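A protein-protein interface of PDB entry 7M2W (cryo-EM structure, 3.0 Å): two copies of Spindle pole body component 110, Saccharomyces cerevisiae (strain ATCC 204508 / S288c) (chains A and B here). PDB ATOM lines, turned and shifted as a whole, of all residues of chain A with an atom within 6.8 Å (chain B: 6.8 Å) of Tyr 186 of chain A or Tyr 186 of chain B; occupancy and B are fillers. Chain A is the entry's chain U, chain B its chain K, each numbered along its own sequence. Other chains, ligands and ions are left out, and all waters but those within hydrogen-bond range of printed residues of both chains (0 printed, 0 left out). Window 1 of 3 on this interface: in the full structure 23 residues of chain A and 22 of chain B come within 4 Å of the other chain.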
ATOM      1  N   ASP A 181     -35.649  -8.373 -24.786  1.00  0.00           N
ATOM      2  CA  ASP A 181     -34.953  -8.810 -23.592  1.00  0.00           C
ATOM      3  C   ASP A 181     -33.689  -7.997 -23.399  1.00  0.00           C
ATOM      4  O   ASP A 181     -33.368  -7.608 -22.272  1.00  0.00           O
ATOM      5  CB  ASP A 181     -34.589 -10.296 -23.682  1.00  0.00           C
ATOM      6  CG  ASP A 181     -35.794 -11.266 -23.559  1.00  0.00           C
ATOM      7  OD1 ASP A 181     -36.862 -10.874 -23.136  1.00  0.00           O
ATOM      8  OD2 ASP A 181     -35.647 -12.429 -23.891  1.00  0.00           O
ATOM      9  N   THR A 182     -33.006  -7.678 -24.498  1.00  0.00           N
ATOM     10  CA  THR A 182     -31.774  -6.920 -24.429  1.00  0.00           C
ATOM     11  C   THR A 182     -32.063  -5.531 -23.885  1.00  0.00           C
ATOM     12  O   THR A 182     -31.322  -5.029 -23.033  1.00  0.00           O
ATOM     13  CB  THR A 182     -31.104  -6.800 -25.813  1.00  0.00           C
ATOM     14  OG1 THR A 182     -30.814  -8.114 -26.328  1.00  0.00           O
ATOM     15  CG2 THR A 182     -29.772  -6.023 -25.660  1.00  0.00           C
ATOM     16  N   LEU A 183     -33.137  -4.904 -24.364  1.00  0.00           N
ATOM     17  CA  LEU A 183     -33.485  -3.572 -23.905  1.00  0.00           C
ATOM     18  C   LEU A 183     -33.881  -3.574 -22.432  1.00  0.00           C
ATOM     19  O   LEU A 183     -33.507  -2.659 -21.685  1.00  0.00           O
ATOM     20  CB  LEU A 183     -34.626  -3.022 -24.764  1.00  0.00           C
ATOM     21  CG  LEU A 183     -34.279  -2.689 -26.251  1.00  0.00           C
ATOM     22  CD1 LEU A 183     -35.562  -2.399 -26.993  1.00  0.00           C
ATOM     23  CD2 LEU A 183     -33.343  -1.461 -26.329  1.00  0.00           C
ATOM     24  N   ASN A 184     -34.587  -4.615 -21.982  1.00  0.00           N
ATOM     25  CA  ASN A 184     -34.968  -4.657 -20.582  1.00  0.00           C
ATOM     26  C   ASN A 184     -33.719  -4.844 -19.710  1.00  0.00           C
ATOM     27  O   ASN A 184     -33.599  -4.235 -18.630  1.00  0.00           O
ATOM     28  CB  ASN A 184     -35.932  -5.803 -20.326  1.00  0.00           C
ATOM     29  CG  ASN A 184     -37.347  -5.627 -20.904  1.00  0.00           C
ATOM     30  OD1 ASN A 184     -37.856  -4.551 -21.262  1.00  0.00           O
ATOM     31  ND2 ASN A 184     -38.020  -6.744 -20.994  1.00  0.00           N
ATOM     32  N   ASN A 185     -32.757  -5.633 -20.214  1.00  0.00           N
ATOM     33  CA  ASN A 185     -31.529  -5.887 -19.483  1.00  0.00           C
ATOM     34  C   ASN A 185     -30.691  -4.628 -19.419  1.00  0.00           C
ATOM     35  O   ASN A 185     -30.049  -4.357 -18.400  1.00  0.00           O
ATOM     36  CB  ASN A 185     -30.732  -6.987 -20.152  1.00  0.00           C
ATOM     37  CG  ASN A 185     -31.345  -8.334 -19.993  1.00  0.00           C
ATOM     38  OD1 ASN A 185     -32.135  -8.588 -19.075  1.00  0.00           O
ATOM     39  ND2 ASN A 185     -30.995  -9.227 -20.882  1.00  0.00           N
ATOM     40  N   TYR A 186     -30.725  -3.843 -20.496  1.00  0.00           N
ATOM     41  CA  TYR A 186     -29.986  -2.601 -20.576  1.00  0.00           C
ATOM     42  C   TYR A 186     -30.429  -1.682 -19.466  1.00  0.00           C
ATOM     43  O   TYR A 186     -29.591  -1.135 -18.749  1.00  0.00           O
ATOM     44  CB  TYR A 186     -30.209  -1.915 -21.922  1.00  0.00           C
ATOM     45  CG  TYR A 186     -29.431  -0.648 -22.089  1.00  0.00           C
ATOM     46  CD1 TYR A 186     -28.167  -0.698 -22.652  1.00  0.00           C
ATOM     47  CD2 TYR A 186     -29.958   0.564 -21.657  1.00  0.00           C
ATOM     48  CE1 TYR A 186     -27.431   0.458 -22.802  1.00  0.00           C
ATOM     49  CE2 TYR A 186     -29.227   1.718 -21.795  1.00  0.00           C
ATOM     50  CZ  TYR A 186     -27.971   1.677 -22.368  1.00  0.00           C
ATOM     51  OH  TYR A 186     -27.248   2.841 -22.505  1.00  0.00           O
ATOM     52  N   ASP A 187     -31.744  -1.515 -19.297  1.00  0.00           N
ATOM     53  CA  ASP A 187     -32.212  -0.618 -18.250  1.00  0.00           C
ATOM     54  C   ASP A 187     -31.843  -1.116 -16.866  1.00  0.00           C
ATOM     55  O   ASP A 187     -31.458  -0.322 -16.004  1.00  0.00           O
ATOM     56  CB  ASP A 187     -33.723  -0.431 -18.322  1.00  0.00           C
ATOM     57  CG  ASP A 187     -34.177   0.454 -19.485  1.00  0.00           C
ATOM     58  OD1 ASP A 187     -33.359   1.118 -20.081  1.00  0.00           O
ATOM     59  OD2 ASP A 187     -35.363   0.495 -19.755  1.00  0.00           O
ATOM     60  N   THR A 188     -31.906  -2.427 -16.652  1.00  0.00           N
ATOM     61  CA  THR A 188     -31.557  -2.957 -15.340  1.00  0.00           C
ATOM     62  C   THR A 188     -30.089  -2.650 -15.046  1.00  0.00           C
ATOM     63  O   THR A 188     -29.722  -2.232 -13.937  1.00  0.00           O
ATOM     64  CB  THR A 188     -31.809  -4.480 -15.275  1.00  0.00           C
ATOM     65  OG1 THR A 188     -33.208  -4.747 -15.493  1.00  0.00           O
ATOM     66  CG2 THR A 188     -31.411  -5.020 -13.905  1.00  0.00           C
ATOM     67  N   LEU A 189     -29.252  -2.854 -16.058  1.00  0.00           N
ATOM     68  CA  LEU A 189     -27.832  -2.618 -15.968  1.00  0.00           C
ATOM     69  C   LEU A 189     -27.522  -1.135 -15.768  1.00  0.00           C
ATOM     70  O   LEU A 189     -26.603  -0.784 -15.017  1.00  0.00           O
ATOM     71  CB  LEU A 189     -27.162  -3.134 -17.239  1.00  0.00           C
ATOM     72  CG  LEU A 189     -25.659  -2.997 -17.343  1.00  0.00           C
ATOM     73  CD1 LEU A 189     -24.928  -3.753 -16.246  1.00  0.00           C
ATOM     74  CD2 LEU A 189     -25.248  -3.486 -18.716  1.00  0.00           C
ATOM     75  N   GLU A 190     -28.242  -0.253 -16.461  1.00  0.00           N
ATOM     76  CA  GLU A 190     -27.986   1.163 -16.294  1.00  0.00           C
ATOM     77  C   GLU A 190     -28.285   1.561 -14.860  1.00  0.00           C
ATOM     78  O   GLU A 190     -27.519   2.309 -14.255  1.00  0.00           O
ATOM     79  CB  GLU A 190     -28.791   2.015 -17.273  1.00  0.00           C
ATOM     80  CG  GLU A 190     -28.399   3.493 -17.255  1.00  0.00           C
ATOM     81  CD  GLU A 190     -29.065   4.276 -18.333  1.00  0.00           C
ATOM     82  OE1 GLU A 190     -30.268   4.312 -18.362  1.00  0.00           O
ATOM     83  OE2 GLU A 190     -28.369   4.823 -19.154  1.00  0.00           O
ATOM     84  N   GLU A 191     -29.353   1.017 -14.272  1.00  0.00           N
ATOM     85  CA  GLU A 191     -29.656   1.380 -12.898  1.00  0.00           C
ATOM     86  C   GLU A 191     -28.520   0.957 -11.964  1.00  0.00           C
ATOM     87  O   GLU A 191     -28.117   1.740 -11.095  1.00  0.00           O
ATOM     88  CB  GLU A 191     -30.977   0.744 -12.463  1.00  0.00           C
ATOM     89  CG  GLU A 191     -32.203   1.341 -13.159  1.00  0.00           C
ATOM     90  CD  GLU A 191     -33.496   0.641 -12.820  1.00  0.00           C
ATOM     91  OE1 GLU A 191     -33.466  -0.308 -12.076  1.00  0.00           O
ATOM     92  OE2 GLU A 191     -34.521   1.043 -13.336  1.00  0.00           O
ATOM     93  N   THR A 193     -25.420   0.670 -12.821  1.00  0.00           N
ATOM     94  CA  THR A 193     -24.322   1.541 -13.187  1.00  0.00           C
ATOM     95  C   THR A 193     -24.448   2.871 -12.457  1.00  0.00           C
ATOM     96  O   THR A 193     -23.465   3.374 -11.904  1.00  0.00           O
ATOM     97  CB  THR A 193     -24.303   1.793 -14.710  1.00  0.00           C
ATOM     98  OG1 THR A 193     -24.166   0.556 -15.406  1.00  0.00           O
ATOM     99  CG2 THR A 193     -23.113   2.656 -15.068  1.00  0.00           C
ATOM    100  N   ASN B 180     -27.306  -6.283 -32.700  1.00  0.00           N
ATOM    101  CA  ASN B 180     -25.896  -6.124 -32.435  1.00  0.00           C
ATOM    102  C   ASN B 180     -25.544  -4.718 -31.969  1.00  0.00           C
ATOM    103  O   ASN B 180     -24.723  -4.570 -31.063  1.00  0.00           O
ATOM    104  CB  ASN B 180     -25.108  -6.530 -33.653  1.00  0.00           C
ATOM    105  CG  ASN B 180     -25.122  -8.029 -33.836  1.00  0.00           C
ATOM    106  OD1 ASN B 180     -25.333  -8.801 -32.888  1.00  0.00           O
ATOM    107  ND2 ASN B 180     -24.903  -8.462 -35.048  1.00  0.00           N
ATOM    108  N   ASP B 181     -26.213  -3.690 -32.490  1.00  0.00           N
ATOM    109  CA  ASP B 181     -25.898  -2.336 -32.056  1.00  0.00           C
ATOM    110  C   ASP B 181     -26.386  -2.108 -30.630  1.00  0.00           C
ATOM    111  O   ASP B 181     -25.724  -1.432 -29.830  1.00  0.00           O
ATOM    112  CB  ASP B 181     -26.534  -1.306 -32.986  1.00  0.00           C
ATOM    113  CG  ASP B 181     -25.880  -1.233 -34.382  1.00  0.00           C
ATOM    114  OD1 ASP B 181     -24.800  -1.748 -34.597  1.00  0.00           O
ATOM    115  OD2 ASP B 181     -26.467  -0.638 -35.266  1.00  0.00           O
ATOM    116  N   THR B 182     -27.528  -2.703 -30.300  1.00  0.00           N
ATOM    117  CA  THR B 182     -28.120  -2.573 -28.985  1.00  0.00           C
ATOM    118  C   THR B 182     -27.155  -3.208 -28.006  1.00  0.00           C
ATOM    119  O   THR B 182     -26.858  -2.629 -26.954  1.00  0.00           O
ATOM    120  CB  THR B 182     -29.482  -3.296 -28.888  1.00  0.00           C
ATOM    121  OG1 THR B 182     -30.397  -2.765 -29.856  1.00  0.00           O
ATOM    122  CG2 THR B 182     -30.083  -3.062 -27.493  1.00  0.00           C
ATOM    123  N   LEU B 183     -26.637  -4.385 -28.380  1.00  0.00           N
ATOM    124  CA  LEU B 183     -25.675  -5.088 -27.569  1.00  0.00           C
ATOM    125  C   LEU B 183     -24.377  -4.317 -27.478  1.00  0.00           C
ATOM    126  O   LEU B 183     -23.814  -4.202 -26.403  1.00  0.00           O
ATOM    127  CB  LEU B 183     -25.416  -6.486 -28.124  1.00  0.00           C
ATOM    128  CG  LEU B 183     -26.576  -7.502 -27.993  1.00  0.00           C
ATOM    129  CD1 LEU B 183     -26.243  -8.736 -28.815  1.00  0.00           C
ATOM    130  CD2 LEU B 183     -26.772  -7.894 -26.513  1.00  0.00           C
ATOM    131  N   ASN B 184     -23.933  -3.661 -28.543  1.00  0.00           N
ATOM    132  CA  ASN B 184     -22.685  -2.937 -28.399  1.00  0.00           C
ATOM    133  C   ASN B 184     -22.821  -1.902 -27.281  1.00  0.00           C
ATOM    134  O   ASN B 184     -21.896  -1.738 -26.469  1.00  0.00           O
ATOM    135  CB  ASN B 184     -22.311  -2.250 -29.704  1.00  0.00           C
ATOM    136  CG  ASN B 184     -21.827  -3.201 -30.783  1.00  0.00           C
ATOM    137  OD1 ASN B 184     -21.358  -4.315 -30.516  1.00  0.00           O
ATOM    138  ND2 ASN B 184     -21.933  -2.773 -32.016  1.00  0.00           N
ATOM    139  N   ASN B 185     -23.990  -1.254 -27.185  1.00  0.00           N
ATOM    140  CA  ASN B 185     -24.190  -0.284 -26.116  1.00  0.00           C
ATOM    141  C   ASN B 185     -24.353  -0.984 -24.764  1.00  0.00           C
ATOM    142  O   ASN B 185     -23.826  -0.514 -23.752  1.00  0.00           O
ATOM    143  CB  ASN B 185     -25.377   0.596 -26.428  1.00  0.00           C
ATOM    144  CG  ASN B 185     -25.071   1.581 -27.534  1.00  0.00           C
ATOM    145  OD1 ASN B 185     -23.911   1.949 -27.782  1.00  0.00           O
ATOM    146  ND2 ASN B 185     -26.092   2.022 -28.216  1.00  0.00           N
ATOM    147  N   TYR B 186     -25.033  -2.128 -24.754  1.00  0.00           N
ATOM    148  CA  TYR B 186     -25.229  -2.920 -23.545  1.00  0.00           C
ATOM    149  C   TYR B 186     -23.896  -3.370 -22.953  1.00  0.00           C
ATOM    150  O   TYR B 186     -23.668  -3.243 -21.749  1.00  0.00           O
ATOM    151  CB  TYR B 186     -26.095  -4.143 -23.838  1.00  0.00           C
ATOM    152  CG  TYR B 186     -26.269  -4.994 -22.669  1.00  0.00           C
ATOM    153  CD1 TYR B 186     -27.243  -4.716 -21.742  1.00  0.00           C
ATOM    154  CD2 TYR B 186     -25.407  -6.043 -22.491  1.00  0.00           C
ATOM    155  CE1 TYR B 186     -27.351  -5.496 -20.616  1.00  0.00           C
ATOM    156  CE2 TYR B 186     -25.503  -6.807 -21.389  1.00  0.00           C
ATOM    157  CZ  TYR B 186     -26.460  -6.551 -20.445  1.00  0.00           C
ATOM    158  OH  TYR B 186     -26.487  -7.329 -19.314  1.00  0.00           O
ATOM    159  N   ASP B 187     -23.030  -3.914 -23.805  1.00  0.00           N
ATOM    160  CA  ASP B 187     -21.734  -4.427 -23.406  1.00  0.00           C
ATOM    161  C   ASP B 187     -20.862  -3.287 -22.922  1.00  0.00           C
ATOM    162  O   ASP B 187     -20.121  -3.449 -21.950  1.00  0.00           O
ATOM    163  CB  ASP B 187     -21.049  -5.120 -24.587  1.00  0.00           C
ATOM    164  CG  ASP B 187     -21.673  -6.466 -25.004  1.00  0.00           C
ATOM    165  OD1 ASP B 187     -22.444  -7.022 -24.269  1.00  0.00           O
ATOM    166  OD2 ASP B 187     -21.352  -6.920 -26.073  1.00  0.00           O
ATOM    167  N   THR B 188     -20.978  -2.122 -23.567  1.00  0.00           N
ATOM    168  CA  THR B 188     -20.227  -0.947 -23.162  1.00  0.00           C
ATOM    169  C   THR B 188     -20.652  -0.580 -21.749  1.00  0.00           C
ATOM    170  O   THR B 188     -19.816  -0.255 -20.898  1.00  0.00           O
ATOM    171  CB  THR B 188     -20.491   0.241 -24.114  1.00  0.00           C
ATOM    172  OG1 THR B 188     -20.063  -0.096 -25.445  1.00  0.00           O
ATOM    173  CG2 THR B 188     -19.727   1.469 -23.646  1.00  0.00           C
ATOM    174  N   LEU B 189     -21.961  -0.642 -21.502  1.00  0.00           N
ATOM    175  CA  LEU B 189     -22.521  -0.342 -20.206  1.00  0.00           C
ATOM    176  C   LEU B 189     -22.042  -1.379 -19.170  1.00  0.00           C
ATOM    177  O   LEU B 189     -21.753  -1.009 -18.022  1.00  0.00           O
ATOM    178  CB  LEU B 189     -24.055  -0.298 -20.313  1.00  0.00           C
ATOM    179  CG  LEU B 189     -24.854   0.128 -19.077  1.00  0.00           C
ATOM    180  CD1 LEU B 189     -24.508   1.538 -18.646  1.00  0.00           C
ATOM    181  CD2 LEU B 189     -26.353   0.015 -19.404  1.00  0.00           C
ATOM    182  N   GLU B 190     -21.939  -2.672 -19.537  1.00  0.00           N
ATOM    183  CA  GLU B 190     -21.420  -3.621 -18.553  1.00  0.00           C
ATOM    184  C   GLU B 190     -19.976  -3.270 -18.212  1.00  0.00           C
ATOM    185  O   GLU B 190     -19.589  -3.339 -17.044  1.00  0.00           O
ATOM    186  CB  GLU B 190     -21.469  -5.099 -18.993  1.00  0.00           C
ATOM    187  CG  GLU B 190     -22.854  -5.760 -19.041  1.00  0.00           C
ATOM    188  CD  GLU B 190     -22.784  -7.241 -19.326  1.00  0.00           C
ATOM    189  OE1 GLU B 190     -21.727  -7.684 -19.694  1.00  0.00           O
ATOM    190  OE2 GLU B 190     -23.772  -7.944 -19.127  1.00  0.00           O
ATOM    191  N   GLU B 191     -19.183  -2.852 -19.207  1.00  0.00           N
ATOM    192  CA  GLU B 191     -17.803  -2.496 -18.913  1.00  0.00           C
ATOM    193  C   GLU B 191     -17.739  -1.288 -17.982  1.00  0.00           C
ATOM    194  O   GLU B 191     -16.929  -1.274 -17.047  1.00  0.00           O
ATOM    195  CB  GLU B 191     -17.015  -2.194 -20.192  1.00  0.00           C
ATOM    196  CG  GLU B 191     -16.721  -3.405 -21.075  1.00  0.00           C
ATOM    197  CD  GLU B 191     -15.962  -3.041 -22.333  1.00  0.00           C
ATOM    198  OE1 GLU B 191     -15.787  -1.870 -22.576  1.00  0.00           O
ATOM    199  OE2 GLU B 191     -15.555  -3.932 -23.041  1.00  0.00           O
ATOM    200  N   THR B 193     -19.943  -0.472 -15.794  1.00  0.00           N
ATOM    201  CA  THR B 193     -20.404  -0.964 -14.511  1.00  0.00           C
ATOM    202  C   THR B 193     -19.257  -1.617 -13.749  1.00  0.00           C
ATOM    203  O   THR B 193     -19.026  -1.312 -12.572  1.00  0.00           O
ATOM    204  CB  THR B 193     -21.542  -1.998 -14.726  1.00  0.00           C
ATOM    205  OG1 THR B 193     -22.640  -1.379 -15.393  1.00  0.00           O
ATOM    206  CG2 THR B 193     -22.044  -2.544 -13.416  1.00  0.00           C
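The side-chain hydroxyl (OG1) of Thr 193 of chain A sits at hydrogen-bond distance from the side-chain hydroxyl (OG1) of Thr 193 of chain B, at 2.5 Å.
The backbone carbonyl oxygen (O) of Leu 189 of chain B lies within hydrogen-bond range of the side-chain hydroxyl (OG1) of Thr 193 of chain B.
The backbone carbonyl oxygen (O) of Leu 189 of chain A sits at hydrogen-bond distance from the side-chain hydroxyl (OG1) of Thr 193 of chain A, 2.8 Å away.
The side-chain amide nitrogen (ND2) of Asn 185 of chain A sits close to the backbone carbonyl oxygen (O) of Asp 181 of chain A (3.2 Å).
The side-chain hydroxyl of Tyr 186 of chain B lies within hydrogen-bond range of the side-chain carboxylate of Glu 190 of chain B.
CG2 of Thr 182 of chain A touches CG2 of Thr 182 of chain B (3.5 Å).
Thr 182 of chain A touches Leu 183 of chain B (CG2 to CD2, 3.6 Å).
CD2 of Leu 183 of chain A touches CG2 of Thr 182 of chain B, at 3.8 Å.
Asn 185 of chain A touches Tyr 186 of chain B (C to CE1, 3.7 Å).
Tyr 186 of chain A touches Asn 185 of chain B.
CA of Tyr 186 of chain A touches CD1 of Tyr 186 of chain B (3.7 Å).
Leu 189 of chain B touches Tyr 186 of chain A (CD2 to O, 3.5 Å).
Leu 189 of chain A touches Tyr 186 of chain B.
CD2 of Leu 189 of chain A touches CG of Leu 189 of chain B (3.7 Å).
Glu 190 of chain B touches Leu 189 of chain A.
Printed residues of chain B within 4 Å of Asn 185 of chain A: Tyr 186 (3.7 Å).
Of chain B, only Asn 185 (3.9 Å), Tyr 186 (3.7 Å) and Leu 189 (3.5 Å) come within 4 Å of Tyr 186 of chain A.
Thr 188 of chain A touches none of the printed residues of chain B.
Printed residues of chain B within 4 Å of Glu 190 of chain A: Leu 189.
Printed residues of chain B within 4 Å of Thr 193 of chain A: Leu 189 (3.4 Å) and Thr 193 (2.5 Å).
Printed residues of chain A within 4 Å of Thr 182 of chain B: Thr 182 and Leu 183.
Of the printed residues of chain A, Tyr 186 of chain B touches Asn 185, Tyr 186 and Leu 189.
Glu 191 of chain B touches none of the printed residues of chain A.
The nearest printed residue of chain A that does not touch Thr 193 of chain B is Glu 190 of chain A (5.8 Å).
Hydrophobic or aromatic side chains of chain B that line the printed part of chain A: Leu 183, Tyr 186 and Leu 189.
Printed residues of chain A that touch a printed residue of chain B: Thr 182, Leu 183, Asn 185, Tyr 186, Leu 189, Glu 190 and Thr 193.
Thr 182 of chain B touches its own counterpart, Thr 182 of chain A.
Thr 182 of chain A touches Leu 183 of chain B, and with the chains exchanged Leu 183 of chain A touches Thr 182 of chain B.
Tyr 186 of chain B touches its own counterpart, Tyr 186 of chain A.
Leu 189 of chain A touches Glu 190 of chain B, and with the chains exchanged Glu 190 of chain A touches Leu 189 of chain B.
Of the 14 pairs that touch across the chains among the printed residues, 14 have their exchanged pair printed and touching as well.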
